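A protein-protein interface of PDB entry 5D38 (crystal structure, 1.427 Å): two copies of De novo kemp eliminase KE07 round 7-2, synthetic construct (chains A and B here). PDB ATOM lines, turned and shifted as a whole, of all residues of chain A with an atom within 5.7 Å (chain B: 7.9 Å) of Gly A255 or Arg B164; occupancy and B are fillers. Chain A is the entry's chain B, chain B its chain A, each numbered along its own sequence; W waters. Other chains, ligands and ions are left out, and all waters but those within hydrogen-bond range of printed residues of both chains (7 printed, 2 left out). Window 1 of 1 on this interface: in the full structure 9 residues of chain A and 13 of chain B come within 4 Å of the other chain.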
ATOM      1  N   GLU A  42      -9.405  36.509  27.300  1.00  0.00           N
ATOM      2  CA  GLU A  42     -10.093  35.253  27.583  1.00  0.00           C
ATOM      3  C   GLU A  42     -10.496  34.477  26.339  1.00  0.00           C
ATOM      4  O   GLU A  42     -11.119  33.415  26.456  1.00  0.00           O
ATOM      5  CB  GLU A  42     -11.355  35.530  28.398  1.00  0.00           C
ATOM      6  CG  GLU A  42     -11.089  36.143  29.760  1.00  0.00           C
ATOM      7  CD  GLU A  42     -10.757  35.111  30.825  1.00  0.00           C
ATOM      8  OE1 GLU A  42      -9.996  34.163  30.533  1.00  0.00           O
ATOM      9  OE2 GLU A  42     -11.265  35.251  31.957  1.00  0.00           O
ATOM     10  N   ILE A  43     -10.158  34.998  25.158  1.00  0.00           N
ATOM     11  CA  ILE A  43     -10.517  34.346  23.892  1.00  0.00           C
ATOM     12  C   ILE A  43      -9.346  33.999  22.967  1.00  0.00           C
ATOM     13  O   ILE A  43      -9.549  33.410  21.895  1.00  0.00           O
ATOM     14  CB  ILE A  43     -11.609  35.135  23.101  1.00  0.00           C
ATOM     15  CG1 ILE A  43     -11.068  36.472  22.576  1.00  0.00           C
ATOM     16  CG2 ILE A  43     -12.858  35.317  23.970  1.00  0.00           C
ATOM     17  CD1 ILE A  43     -11.977  37.129  21.559  1.00  0.00           C
ATOM     18  N   ARG A 236     -10.247  33.475  17.730  1.00  0.00           N
ATOM     19  CA  ARG A 236     -10.113  32.027  17.758  1.00  0.00           C
ATOM     20  C   ARG A 236      -9.968  31.462  16.342  1.00  0.00           C
ATOM     21  O   ARG A 236      -9.107  30.625  16.096  1.00  0.00           O
ATOM     22  CB  ARG A 236     -11.280  31.381  18.488  1.00  0.00           C
ATOM     23  CG  ARG A 236     -11.163  29.873  18.528  1.00  0.00           C
ATOM     24  CD  ARG A 236     -12.187  29.251  19.449  1.00  0.00           C
ATOM     25  NE  ARG A 236     -11.856  27.856  19.709  1.00  0.00           N
ATOM     26  CZ  ARG A 236     -12.398  27.144  20.689  1.00  0.00           C
ATOM     27  NH1 ARG A 236     -13.294  27.700  21.491  1.00  0.00           N
ATOM     28  NH2 ARG A 236     -12.034  25.882  20.865  1.00  0.00           N
ATOM     29  N   LEU A 251      -2.522  28.140  21.661  1.00  0.00           N
ATOM     30  CA  LEU A 251      -3.943  27.851  21.730  1.00  0.00           C
ATOM     31  C   LEU A 251      -4.464  27.721  23.159  1.00  0.00           C
ATOM     32  O   LEU A 251      -5.653  27.459  23.344  1.00  0.00           O
ATOM     33  CB  LEU A 251      -4.261  26.563  20.972  1.00  0.00           C
ATOM     34  CG  LEU A 251      -3.705  26.463  19.552  1.00  0.00           C
ATOM     35  CD1 LEU A 251      -3.965  25.059  19.020  1.00  0.00           C
ATOM     36  CD2 LEU A 251      -4.361  27.499  18.670  1.00  0.00           C
ATOM     37  N   GLU A 252      -3.596  27.933  24.148  1.00  0.00           N
ATOM     38  CA  GLU A 252      -3.939  27.643  25.549  1.00  0.00           C
ATOM     39  C   GLU A 252      -5.076  28.487  26.082  1.00  0.00           C
ATOM     40  O   GLU A 252      -5.774  28.075  27.013  1.00  0.00           O
ATOM     41  CB  GLU A 252      -2.724  27.797  26.467  1.00  0.00           C
ATOM     42  CG  GLU A 252      -1.622  26.785  26.216  1.00  0.00           C
ATOM     43  CD  GLU A 252      -0.589  27.314  25.259  1.00  0.00           C
ATOM     44  OE1 GLU A 252      -0.881  28.301  24.562  1.00  0.00           O
ATOM     45  OE2 GLU A 252       0.520  26.759  25.209  1.00  0.00           O
ATOM     46  N   GLY A 253      -5.256  29.669  25.502  1.00  0.00           N
ATOM     47  CA  GLY A 253      -6.243  30.602  26.000  1.00  0.00           C
ATOM     48  C   GLY A 253      -7.575  30.529  25.287  1.00  0.00           C
ATOM     49  O   GLY A 253      -8.519  31.222  25.675  1.00  0.00           O
ATOM     50  N   LEU A 254      -7.669  29.700  24.249  1.00  0.00           N
ATOM     51  CA  LEU A 254      -8.928  29.576  23.507  1.00  0.00           C
ATOM     52  C   LEU A 254     -10.043  29.025  24.384  1.00  0.00           C
ATOM     53  O   LEU A 254      -9.821  28.112  25.177  1.00  0.00           O
ATOM     54  CB  LEU A 254      -8.762  28.681  22.279  1.00  0.00           C
ATOM     55  CG  LEU A 254      -7.755  29.120  21.209  1.00  0.00           C
ATOM     56  CD1 LEU A 254      -7.789  28.174  20.031  1.00  0.00           C
ATOM     57  CD2 LEU A 254      -8.005  30.550  20.749  1.00  0.00           C
ATOM     58  N   GLY A 255     -11.239  29.587  24.257  1.00  0.00           N
ATOM     59  CA  GLY A 255     -12.393  29.044  24.956  1.00  0.00           C
ATOM     60  C   GLY A 255     -12.416  29.180  26.472  1.00  0.00           C
ATOM     61  O   GLY A 255     -13.204  28.491  27.139  1.00  0.00           O
ATOM     62  N   SER A 256     -11.590  30.063  27.035  1.00  0.00           N
ATOM     63  CA  SER A 256     -11.498  30.191  28.493  1.00  0.00           C
ATOM     64  C   SER A 256     -12.833  30.491  29.183  1.00  0.00           C
ATOM     65  O   SER A 256     -13.028  30.122  30.348  1.00  0.00           O
ATOM     66  CB  SER A 256     -10.480  31.262  28.883  1.00  0.00           C
ATOM     67  OG  SER A 256      -9.169  30.904  28.490  1.00  0.00           O
ATOM     68  N   LEU A 257     -13.746  31.144  28.469  1.00  0.00           N
ATOM     69  CA  LEU A 257     -15.042  31.506  29.039  1.00  0.00           C
ATOM     70  C   LEU A 257     -16.052  30.382  28.886  1.00  0.00           C
ATOM     71  O   LEU A 257     -17.135  30.421  29.479  1.00  0.00           O
ATOM     72  CB  LEU A 257     -15.567  32.775  28.367  1.00  0.00           C
ATOM     73  CG  LEU A 257     -14.646  33.988  28.470  1.00  0.00           C
ATOM     74  CD1 LEU A 257     -15.219  35.179  27.704  1.00  0.00           C
ATOM     75  CD2 LEU A 257     -14.404  34.347  29.933  1.00  0.00           C
ATOM     76  N   GLU A 258     -15.688  29.374  28.097  1.00  0.00           N
ATOM     77  CA  GLU A 258     -16.599  28.291  27.768  1.00  0.00           C
ATOM     78  C   GLU A 258     -16.524  27.169  28.783  1.00  0.00           C
ATOM     79  O   GLU A 258     -15.499  26.965  29.439  1.00  0.00           O
ATOM     80  CB  GLU A 258     -16.302  27.763  26.372  1.00  0.00           C
ATOM     81  CG  GLU A 258     -16.534  28.811  25.298  1.00  0.00           C
ATOM     82  CD  GLU A 258     -16.117  28.353  23.924  1.00  0.00           C
ATOM     83  OE1 GLU A 258     -15.444  27.309  23.813  1.00  0.00           O
ATOM     84  OE2 GLU A 258     -16.468  29.047  22.947  1.00  0.00           O
ATOM     85  N   HIS A 259     -17.616  26.430  28.912  1.00  0.00           N
ATOM     86  CA  HIS A 259     -17.704  25.416  29.949  1.00  0.00           C
ATOM     87  C   HIS A 259     -18.413  24.200  29.406  1.00  0.00           C
ATOM     88  O   HIS A 259     -18.919  24.199  28.281  1.00  0.00           O
ATOM     89  CB  HIS A 259     -18.456  25.960  31.163  1.00  0.00           C
ATOM     90  CG  HIS A 259     -19.822  26.469  30.833  1.00  0.00           C
ATOM     91  ND1 HIS A 259     -20.877  25.630  30.551  1.00  0.00           N
ATOM     92  CD2 HIS A 259     -20.298  27.732  30.705  1.00  0.00           C
ATOM     93  CE1 HIS A 259     -21.951  26.353  30.281  1.00  0.00           C
ATOM     94  NE2 HIS A 259     -21.624  27.630  30.364  1.00  0.00           N
ATOM     95  N   HIS A 260     -18.449  23.151  30.217  1.00  0.00           N
ATOM     96  CA  HIS A 260     -18.979  21.881  29.746  1.00  0.00           C
ATOM     97  C   HIS A 260     -20.410  21.610  30.185  1.00  0.00           C
ATOM     98  O   HIS A 260     -20.904  20.494  30.062  1.00  0.00           O
ATOM     99  CB  HIS A 260     -18.059  20.732  30.147  1.00  0.00           C
ATOM    100  CG  HIS A 260     -17.882  20.591  31.623  1.00  0.00           C
ATOM    101  ND1 HIS A 260     -17.299  21.561  32.402  1.00  0.00           N
ATOM    102  CD2 HIS A 260     -18.242  19.591  32.470  1.00  0.00           C
ATOM    103  CE1 HIS A 260     -17.290  21.167  33.665  1.00  0.00           C
ATOM    104  NE2 HIS A 260     -17.852  19.973  33.726  1.00  0.00           N
ATOM    105  N   ALA B 107      -4.237  18.165  25.206  1.00  0.00           N
ATOM    106  CA  ALA B 107      -4.946  19.026  26.160  1.00  0.00           C
ATOM    107  C   ALA B 107      -4.059  20.142  26.707  1.00  0.00           C
ATOM    108  O   ALA B 107      -4.516  21.257  26.942  1.00  0.00           O
ATOM    109  CB  ALA B 107      -5.520  18.200  27.315  1.00  0.00           C
ATOM    110  N   ASN B 110      -4.070  22.599  23.907  1.00  0.00           N
ATOM    111  CA  ASN B 110      -5.400  23.112  23.609  1.00  0.00           C
ATOM    112  C   ASN B 110      -6.363  22.613  24.677  1.00  0.00           C
ATOM    113  O   ASN B 110      -7.063  21.621  24.459  1.00  0.00           O
ATOM    114  CB  ASN B 110      -5.835  22.629  22.222  1.00  0.00           C
ATOM    115  CG  ASN B 110      -7.116  23.282  21.749  1.00  0.00           C
ATOM    116  OD1 ASN B 110      -7.628  24.209  22.383  1.00  0.00           O
ATOM    117  ND2 ASN B 110      -7.656  22.788  20.640  1.00  0.00           N
ATOM    118  N   PRO B 111      -6.394  23.287  25.840  1.00  0.00           N
ATOM    119  CA  PRO B 111      -7.223  22.780  26.948  1.00  0.00           C
ATOM    120  C   PRO B 111      -8.727  22.730  26.642  1.00  0.00           C
ATOM    121  O   PRO B 111      -9.461  22.009  27.327  1.00  0.00           O
ATOM    122  CB  PRO B 111      -6.905  23.748  28.105  1.00  0.00           C
ATOM    123  CG  PRO B 111      -5.510  24.259  27.816  1.00  0.00           C
ATOM    124  CD  PRO B 111      -5.464  24.352  26.292  1.00  0.00           C
ATOM    125  N   SER B 112      -9.168  23.497  25.649  1.00  0.00           N
ATOM    126  CA  SER B 112     -10.538  23.443  25.142  1.00  0.00           C
ATOM    127  C   SER B 112     -10.998  22.020  24.836  1.00  0.00           C
ATOM    128  O   SER B 112     -12.179  21.706  24.966  1.00  0.00           O
ATOM    129  CB  SER B 112     -10.672  24.305  23.877  1.00  0.00           C
ATOM    130  OG  SER B 112     -11.986  24.249  23.342  1.00  0.00           O
ATOM    131  N   LEU B 113     -10.065  21.165  24.419  1.00  0.00           N
ATOM    132  CA  LEU B 113     -10.396  19.783  24.084  1.00  0.00           C
ATOM    133  C   LEU B 113     -11.028  19.037  25.260  1.00  0.00           C
ATOM    134  O   LEU B 113     -11.901  18.196  25.068  1.00  0.00           O
ATOM    135  CB  LEU B 113      -9.150  19.037  23.616  1.00  0.00           C
ATOM    136  CG  LEU B 113      -8.601  19.378  22.231  1.00  0.00           C
ATOM    137  CD1 LEU B 113      -7.332  18.593  21.951  1.00  0.00           C
ATOM    138  CD2 LEU B 113      -9.645  19.101  21.167  1.00  0.00           C
ATOM    139  N   ILE B 114     -10.578  19.348  26.471  1.00  0.00           N
ATOM    140  CA  ILE B 114     -11.155  18.763  27.678  1.00  0.00           C
ATOM    141  C   ILE B 114     -12.634  19.111  27.750  1.00  0.00           C
ATOM    142  O   ILE B 114     -13.489  18.232  27.900  1.00  0.00           O
ATOM    143  CB  ILE B 114     -10.443  19.271  28.939  1.00  0.00           C
ATOM    144  CG1 ILE B 114      -8.988  18.792  28.964  1.00  0.00           C
ATOM    145  CG2 ILE B 114     -11.201  18.810  30.180  1.00  0.00           C
ATOM    146  CD1 ILE B 114      -8.107  19.514  29.967  1.00  0.00           C
ATOM    147  N   THR B 115     -12.928  20.402  27.607  1.00  0.00           N
ATOM    148  CA  THR B 115     -14.295  20.898  27.684  1.00  0.00           C
ATOM    149  C   THR B 115     -15.181  20.321  26.590  1.00  0.00           C
ATOM    150  O   THR B 115     -16.337  19.994  26.838  1.00  0.00           O
ATOM    151  CB  THR B 115     -14.299  22.419  27.604  1.00  0.00           C
ATOM    152  OG1 THR B 115     -13.322  22.930  28.504  1.00  0.00           O
ATOM    153  CG2 THR B 115     -15.651  23.001  27.975  1.00  0.00           C
ATOM    154  N   GLN B 116     -14.632  20.190  25.386  1.00  0.00           N
ATOM    155  CA  GLN B 116     -15.408  19.665  24.256  1.00  0.00           C
ATOM    156  C   GLN B 116     -15.880  18.235  24.509  1.00  0.00           C
ATOM    157  O   GLN B 116     -17.046  17.914  24.277  1.00  0.00           O
ATOM    158  CB  GLN B 116     -14.600  19.727  22.956  1.00  0.00           C
ATOM    159  CG  GLN B 116     -14.273  21.139  22.504  1.00  0.00           C
ATOM    160  CD  GLN B 116     -13.297  21.154  21.346  1.00  0.00           C
ATOM    161  OE1 GLN B 116     -13.315  20.270  20.490  1.00  0.00           O
ATOM    162  NE2 GLN B 116     -12.437  22.160  21.315  1.00  0.00           N
ATOM    163  N   ILE B 117     -14.987  17.381  25.000  1.00  0.00           N
ATOM    164  CA  ILE B 117     -15.376  16.015  25.313  1.00  0.00           C
ATOM    165  C   ILE B 117     -16.301  15.975  26.525  1.00  0.00           C
ATOM    166  O   ILE B 117     -17.293  15.251  26.518  1.00  0.00           O
ATOM    167  CB  ILE B 117     -14.144  15.102  25.503  1.00  0.00           C
ATOM    168  CG1 ILE B 117     -13.405  14.932  24.172  1.00  0.00           C
ATOM    169  CG2 ILE B 117     -14.544  13.734  26.044  1.00  0.00           C
ATOM    170  CD1 ILE B 117     -14.173  14.108  23.157  1.00  0.00           C
ATOM    171  N   ALA B 118     -16.008  16.777  27.546  1.00  0.00           N
ATOM    172  CA  ALA B 118     -16.852  16.795  28.738  1.00  0.00           C
ATOM    173  C   ALA B 118     -18.270  17.275  28.428  1.00  0.00           C
ATOM    174  O   ALA B 118     -19.235  16.801  29.016  1.00  0.00           O
ATOM    175  CB  ALA B 118     -16.225  17.628  29.842  1.00  0.00           C
ATOM    176  N   GLN B 119     -18.397  18.216  27.499  1.00  0.00           N
ATOM    177  CA  GLN B 119     -19.711  18.728  27.135  1.00  0.00           C
ATOM    178  C   GLN B 119     -20.535  17.648  26.452  1.00  0.00           C
ATOM    179  O   GLN B 119     -21.733  17.528  26.696  1.00  0.00           O
ATOM    180  CB  GLN B 119     -19.578  19.946  26.220  1.00  0.00           C
ATOM    181  CG  GLN B 119     -20.910  20.522  25.783  1.00  0.00           C
ATOM    182  CD  GLN B 119     -20.762  21.849  25.061  1.00  0.00           C
ATOM    183  OE1 GLN B 119     -20.128  22.778  25.567  1.00  0.00           O
ATOM    184  NE2 GLN B 119     -21.348  21.944  23.872  1.00  0.00           N
ATOM    185  N   SER B 123     -18.032  14.881  32.149  1.00  0.00           N
ATOM    186  CA  SER B 123     -16.710  14.956  32.783  1.00  0.00           C
ATOM    187  C   SER B 123     -16.122  13.581  33.081  1.00  0.00           C
ATOM    188  O   SER B 123     -14.912  13.381  33.007  1.00  0.00           O
ATOM    189  CB  SER B 123     -16.774  15.760  34.080  1.00  0.00           C
ATOM    190  OG  SER B 123     -17.058  17.121  33.826  1.00  0.00           O
ATOM    191  N   VAL B 126     -13.648  11.901  30.776  1.00  0.00           N
ATOM    192  CA  VAL B 126     -12.385  12.590  30.512  1.00  0.00           C
ATOM    193  C   VAL B 126     -11.362  12.397  31.610  1.00  0.00           C
ATOM    194  O   VAL B 126     -11.587  12.771  32.764  1.00  0.00           O
ATOM    195  CB  VAL B 126     -12.574  14.113  30.365  1.00  0.00           C
ATOM    196  CG1 VAL B 126     -11.223  14.779  30.101  1.00  0.00           C
ATOM    197  CG2 VAL B 126     -13.559  14.432  29.268  1.00  0.00           C
ATOM    198  N   VAL B 128      -7.253  13.361  32.419  1.00  0.00           N
ATOM    199  CA  VAL B 128      -6.040  14.047  31.992  1.00  0.00           C
ATOM    200  C   VAL B 128      -4.839  13.421  32.687  1.00  0.00           C
ATOM    201  O   VAL B 128      -4.801  13.332  33.923  1.00  0.00           O
ATOM    202  CB  VAL B 128      -6.080  15.574  32.231  1.00  0.00           C
ATOM    203  CG1 VAL B 128      -4.774  16.194  31.800  1.00  0.00           C
ATOM    204  CG2 VAL B 128      -7.214  16.212  31.436  1.00  0.00           C
ATOM    205  N   TRP B 157      -1.624  24.042  36.015  1.00  0.00           N
ATOM    206  CA  TRP B 157      -2.296  23.133  35.099  1.00  0.00           C
ATOM    207  C   TRP B 157      -3.358  22.297  35.812  1.00  0.00           C
ATOM    208  O   TRP B 157      -4.435  22.085  35.274  1.00  0.00           O
ATOM    209  CB  TRP B 157      -1.250  22.276  34.380  1.00  0.00           C
ATOM    210  CG  TRP B 157      -1.777  21.313  33.358  1.00  0.00           C
ATOM    211  CD1 TRP B 157      -1.410  20.008  33.219  1.00  0.00           C
ATOM    212  CD2 TRP B 157      -2.740  21.567  32.325  1.00  0.00           C
ATOM    213  NE1 TRP B 157      -2.082  19.429  32.176  1.00  0.00           N
ATOM    214  CE2 TRP B 157      -2.904  20.365  31.604  1.00  0.00           C
ATOM    215  CE3 TRP B 157      -3.476  22.692  31.930  1.00  0.00           C
ATOM    216  CZ2 TRP B 157      -3.789  20.250  30.521  1.00  0.00           C
ATOM    217  CZ3 TRP B 157      -4.342  22.574  30.867  1.00  0.00           C
ATOM    218  CH2 TRP B 157      -4.490  21.367  30.172  1.00  0.00           C
ATOM    219  N   VAL B 158      -3.079  21.868  37.038  1.00  0.00           N
ATOM    220  CA  VAL B 158      -4.072  21.144  37.809  1.00  0.00           C
ATOM    221  C   VAL B 158      -5.371  21.948  37.947  1.00  0.00           C
ATOM    222  O   VAL B 158      -6.456  21.417  37.714  1.00  0.00           O
ATOM    223  CB  VAL B 158      -3.526  20.730  39.177  1.00  0.00           C
ATOM    224  CG1 VAL B 158      -4.657  20.321  40.112  1.00  0.00           C
ATOM    225  CG2 VAL B 158      -2.526  19.586  39.017  1.00  0.00           C
ATOM    226  N   VAL B 159      -5.252  23.221  38.299  1.00  0.00           N
ATOM    227  CA  VAL B 159      -6.430  24.066  38.471  1.00  0.00           C
ATOM    228  C   VAL B 159      -7.168  24.215  37.148  1.00  0.00           C
ATOM    229  O   VAL B 159      -8.392  24.119  37.092  1.00  0.00           O
ATOM    230  CB  VAL B 159      -6.026  25.427  39.066  1.00  0.00           C
ATOM    231  CG1 VAL B 159      -7.203  26.386  39.112  1.00  0.00           C
ATOM    232  CG2 VAL B 159      -5.443  25.223  40.454  1.00  0.00           C
ATOM    233  N   GLU B 160      -6.410  24.400  36.076  1.00  0.00           N
ATOM    234  CA  GLU B 160      -7.013  24.610  34.767  1.00  0.00           C
ATOM    235  C   GLU B 160      -7.717  23.344  34.286  1.00  0.00           C
ATOM    236  O   GLU B 160      -8.785  23.409  33.684  1.00  0.00           O
ATOM    237  CB  GLU B 160      -5.954  25.065  33.758  1.00  0.00           C
ATOM    238  CG  GLU B 160      -6.504  25.456  32.384  1.00  0.00           C
ATOM    239  CD  GLU B 160      -7.313  26.747  32.406  1.00  0.00           C
ATOM    240  OE1 GLU B 160      -8.240  26.892  31.584  1.00  0.00           O
ATOM    241  OE2 GLU B 160      -7.004  27.618  33.238  1.00  0.00           O
ATOM    242  N   VAL B 161      -7.124  22.189  34.573  1.00  0.00           N
ATOM    243  CA  VAL B 161      -7.700  20.911  34.182  1.00  0.00           C
ATOM    244  C   VAL B 161      -9.081  20.720  34.826  1.00  0.00           C
ATOM    245  O   VAL B 161     -10.050  20.321  34.158  1.00  0.00           O
ATOM    246  CB  VAL B 161      -6.730  19.743  34.494  1.00  0.00           C
ATOM    247  CG1 VAL B 161      -7.459  18.395  34.487  1.00  0.00           C
ATOM    248  CG2 VAL B 161      -5.572  19.738  33.502  1.00  0.00           C
ATOM    249  N   GLU B 162      -9.191  21.059  36.111  1.00  0.00           N
ATOM    250  CA  GLU B 162     -10.486  20.975  36.780  1.00  0.00           C
ATOM    251  C   GLU B 162     -11.484  21.987  36.189  1.00  0.00           C
ATOM    252  O   GLU B 162     -12.608  21.618  35.888  1.00  0.00           O
ATOM    253  CB  GLU B 162     -10.352  21.144  38.303  1.00  0.00           C
ATOM    254  CG  GLU B 162     -11.696  21.041  39.021  1.00  0.00           C
ATOM    255  CD  GLU B 162     -11.587  20.978  40.529  1.00  0.00           C
ATOM    256  OE1 GLU B 162     -10.484  20.724  41.045  1.00  0.00           O
ATOM    257  OE2 GLU B 162     -12.613  21.195  41.203  1.00  0.00           O
ATOM    258  N   LYS B 163     -11.043  23.232  36.008  1.00  0.00           N
ATOM    259  CA  LYS B 163     -11.895  24.287  35.449  1.00  0.00           C
ATOM    260  C   LYS B 163     -12.484  23.889  34.090  1.00  0.00           C
ATOM    261  O   LYS B 163     -13.664  24.138  33.817  1.00  0.00           O
ATOM    262  CB  LYS B 163     -11.086  25.582  35.308  1.00  0.00           C
ATOM    263  CG  LYS B 163     -11.834  26.749  34.693  1.00  0.00           C
ATOM    264  CD  LYS B 163     -10.938  27.984  34.646  1.00  0.00           C
ATOM    265  CE  LYS B 163     -11.558  29.078  33.794  1.00  0.00           C
ATOM    266  NZ  LYS B 163     -10.608  30.198  33.528  1.00  0.00           N
ATOM    267  N   ARG B 164     -11.657  23.262  33.251  1.00  0.00           N
ATOM    268  CA  ARG B 164     -12.053  22.909  31.887  1.00  0.00           C
ATOM    269  C   ARG B 164     -13.019  21.723  31.814  1.00  0.00           C
ATOM    270  O   ARG B 164     -13.620  21.464  30.779  1.00  0.00           O
ATOM    271  CB  ARG B 164     -10.812  22.610  31.040  1.00  0.00           C
ATOM    272  CG  ARG B 164      -9.934  23.809  30.751  1.00  0.00           C
ATOM    273  CD  ARG B 164     -10.525  24.725  29.698  1.00  0.00           C
ATOM    274  NE  ARG B 164      -9.568  25.791  29.420  1.00  0.00           N
ATOM    275  CZ  ARG B 164      -9.549  26.523  28.311  1.00  0.00           C
ATOM    276  NH1 ARG B 164     -10.444  26.313  27.364  1.00  0.00           N
ATOM    277  NH2 ARG B 164      -8.620  27.455  28.147  1.00  0.00           N
ATOM    278  N   GLY B 165     -13.163  20.983  32.905  1.00  0.00           N
ATOM    279  CA  GLY B 165     -14.141  19.903  32.933  1.00  0.00           C
ATOM    280  C   GLY B 165     -13.646  18.466  32.995  1.00  0.00           C
ATOM    281  O   GLY B 165     -14.427  17.547  32.774  1.00  0.00           O
ATOM    282  N   ALA B 166     -12.376  18.252  33.314  1.00  0.00           N
ATOM    283  CA  ALA B 166     -11.887  16.875  33.420  1.00  0.00           C
ATOM    284  C   ALA B 166     -12.506  16.152  34.617  1.00  0.00           C
ATOM    285  O   ALA B 166     -12.904  16.778  35.606  1.00  0.00           O
ATOM    286  CB  ALA B 166     -10.374  16.848  33.509  1.00  0.00           C
ATOM    287  N   GLY B 167     -12.618  14.838  34.495  1.00  0.00           N
ATOM    288  CA  GLY B 167     -13.206  14.009  35.543  1.00  0.00           C
ATOM    289  C   GLY B 167     -12.211  13.485  36.564  1.00  0.00           C
ATOM    290  O   GLY B 167     -12.529  13.338  37.744  1.00  0.00           O
ATOM    291  N   LEU B 197     -10.732  16.885  42.283  1.00  0.00           N
ATOM    292  CA  LEU B 197     -10.888  15.722  41.426  1.00  0.00           C
ATOM    293  C   LEU B 197     -10.167  14.509  42.003  1.00  0.00           C
ATOM    294  O   LEU B 197      -9.224  14.653  42.782  1.00  0.00           O
ATOM    295  CB  LEU B 197     -10.325  15.999  40.031  1.00  0.00           C
ATOM    296  CG  LEU B 197     -10.966  17.086  39.174  1.00  0.00           C
ATOM    297  CD1 LEU B 197     -10.240  17.126  37.834  1.00  0.00           C
ATOM    298  CD2 LEU B 197     -12.452  16.806  38.963  1.00  0.00           C
HETATM  299  O   HOH W   1     -14.306  25.192  25.076  1.00  0.00           O
HETATM  300  O   HOH W   2     -13.223  25.591  27.621  1.00  0.00           O
HETATM  301  O   HOH W   3     -21.718  25.293  27.182  1.00  0.00           O
HETATM  302  O   HOH W   4     -13.609  25.777  30.402  1.00  0.00           O
HETATM  303  O   HOH W   5      -9.705  28.923  31.198  1.00  0.00           O
HETATM  304  O   HOH W   6     -15.733  23.907  32.102  1.00  0.00           O
HETATM  305  O   HOH W   7      -9.473  25.292  20.153  1.00  0.00           O
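The side-chain hydroxyl of Ser B112 sits at hydrogen-bond distance from the guanidinium group of Arg A236, 3.0 Å away. O of His A259 lies close to OE1 of Gln B119. NH2 of Arg B164 is in hydrogen-bond range of O of Glu A252 (3.1 Å). The backbone carbonyl oxygen of Leu A254 sits at hydrogen-bond distance from the guanidinium group of Arg B164. The side-chain hydroxyl (OG) of Ser B123 lies within hydrogen-bond range of a ring nitrogen (NE2) of His A260 (3.0 Å).
The side-chain hydroxyl (OG) of Ser B123 sits at hydrogen-bond distance from the backbone carbonyl oxygen (O) of Gly B165. The side-chain hydroxyl (OG1) of Thr B115 sits at hydrogen-bond distance from the backbone carbonyl oxygen (O) of Arg B164 (2.7 Å). The backbone carbonyl oxygen of Ser B123 sits at hydrogen-bond distance from the backbone NH of Gly B167 (3.1 Å).
Among the printed residues, merely in contact across the chains: His A259 with Thr B115 (3.3 Å), His A260 with Gly B165 (3.5 Å), Ser A256 with Arg B164 (3.5 Å), Gly A255 with Arg B164 (3.5 Å), His A260 with Thr B115 (3.6 Å), His A260 with Ala B118 (3.6 Å), His A260 with Gln B119 (3.6 Å), Glu A252 with Pro B111 (3.7 Å), Arg A236 with Gln B116 (3.8 Å), Ser A256 with Lys B163 (3.9 Å) and Leu A251 with Asn B110 (3.9 Å).
Glu A42 touches none of the printed residues of chain B. Of the printed residues of chain B, Leu A251 touches Asn B110 (3.9 Å). Of chain B, only Arg B164 (3.5 Å) comes within 4 Å of Gly A255. Ser A256 touches two residues of chain B. Printed residues of chain A within 4 Å of Pro B111: Glu A252. Of the printed residues of chain A, Ser B112 touches Arg A236. Printed residues of chain A within 4 Å of Gln B119: His A259 (3.3 Å) and His A260 (3.6 Å). Of the printed residues of chain A, Lys B163 touches Ser A256 (3.9 Å). Arg B164 touches just these residues of chain A: Glu A252 (3.1 Å), Leu A254 (2.9 Å), Gly A255 (3.5 Å) and Ser A256 (3.5 Å). The nearest printed residue of chain B that does not touch Gly A255 is Ser B112 (5.1 Å). The nearest residue of chain A that does not touch Arg B164 is His A260 (4.02 Å).
Of the 26 printed residues of chain B, 11 touch a printed residue of chain A. Hydrophobic or aromatic side chains of chain B within 4 Å of the printed part of chain A: Pro B111 and Ala B118. Along chain B the printed residues that touch a printed residue of chain A span positions 110 to 165. Of the 13 printed residues of chain A, 8 touch a printed residue of chain B. Hydrophobic or aromatic side chains of chain A that line the printed part of chain B: His A260. Among the printed residues, no Asp or Glu carboxylate lies within 4 Å of a Lys or Arg side-chain nitrogen of the other chain.
No position is printed for both chains. Of the 16 pairs that touch across the chains among the printed residues, none has its exchanged pair printed and touching as well.
Water W6 lies within hydrogen-bond range of the backbone carbonyl oxygen of Lys B163 (2.7 Å), a ring nitrogen (ND1) of His A260 (2.8 Å) and the backbone carbonyl oxygen of Arg B164 (3.5 Å). Water W2 lies within hydrogen-bond range of OG1 of Thr B115 (2.8 Å), NH1 of Arg B164 (2.9 Å), O of Gly A255 (2.9 Å) and O of Glu A258 (3.2 Å). Water W3 bridges O of His A259 (3.2 Å) and OE1 of Gln B119 (3.4 Å).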
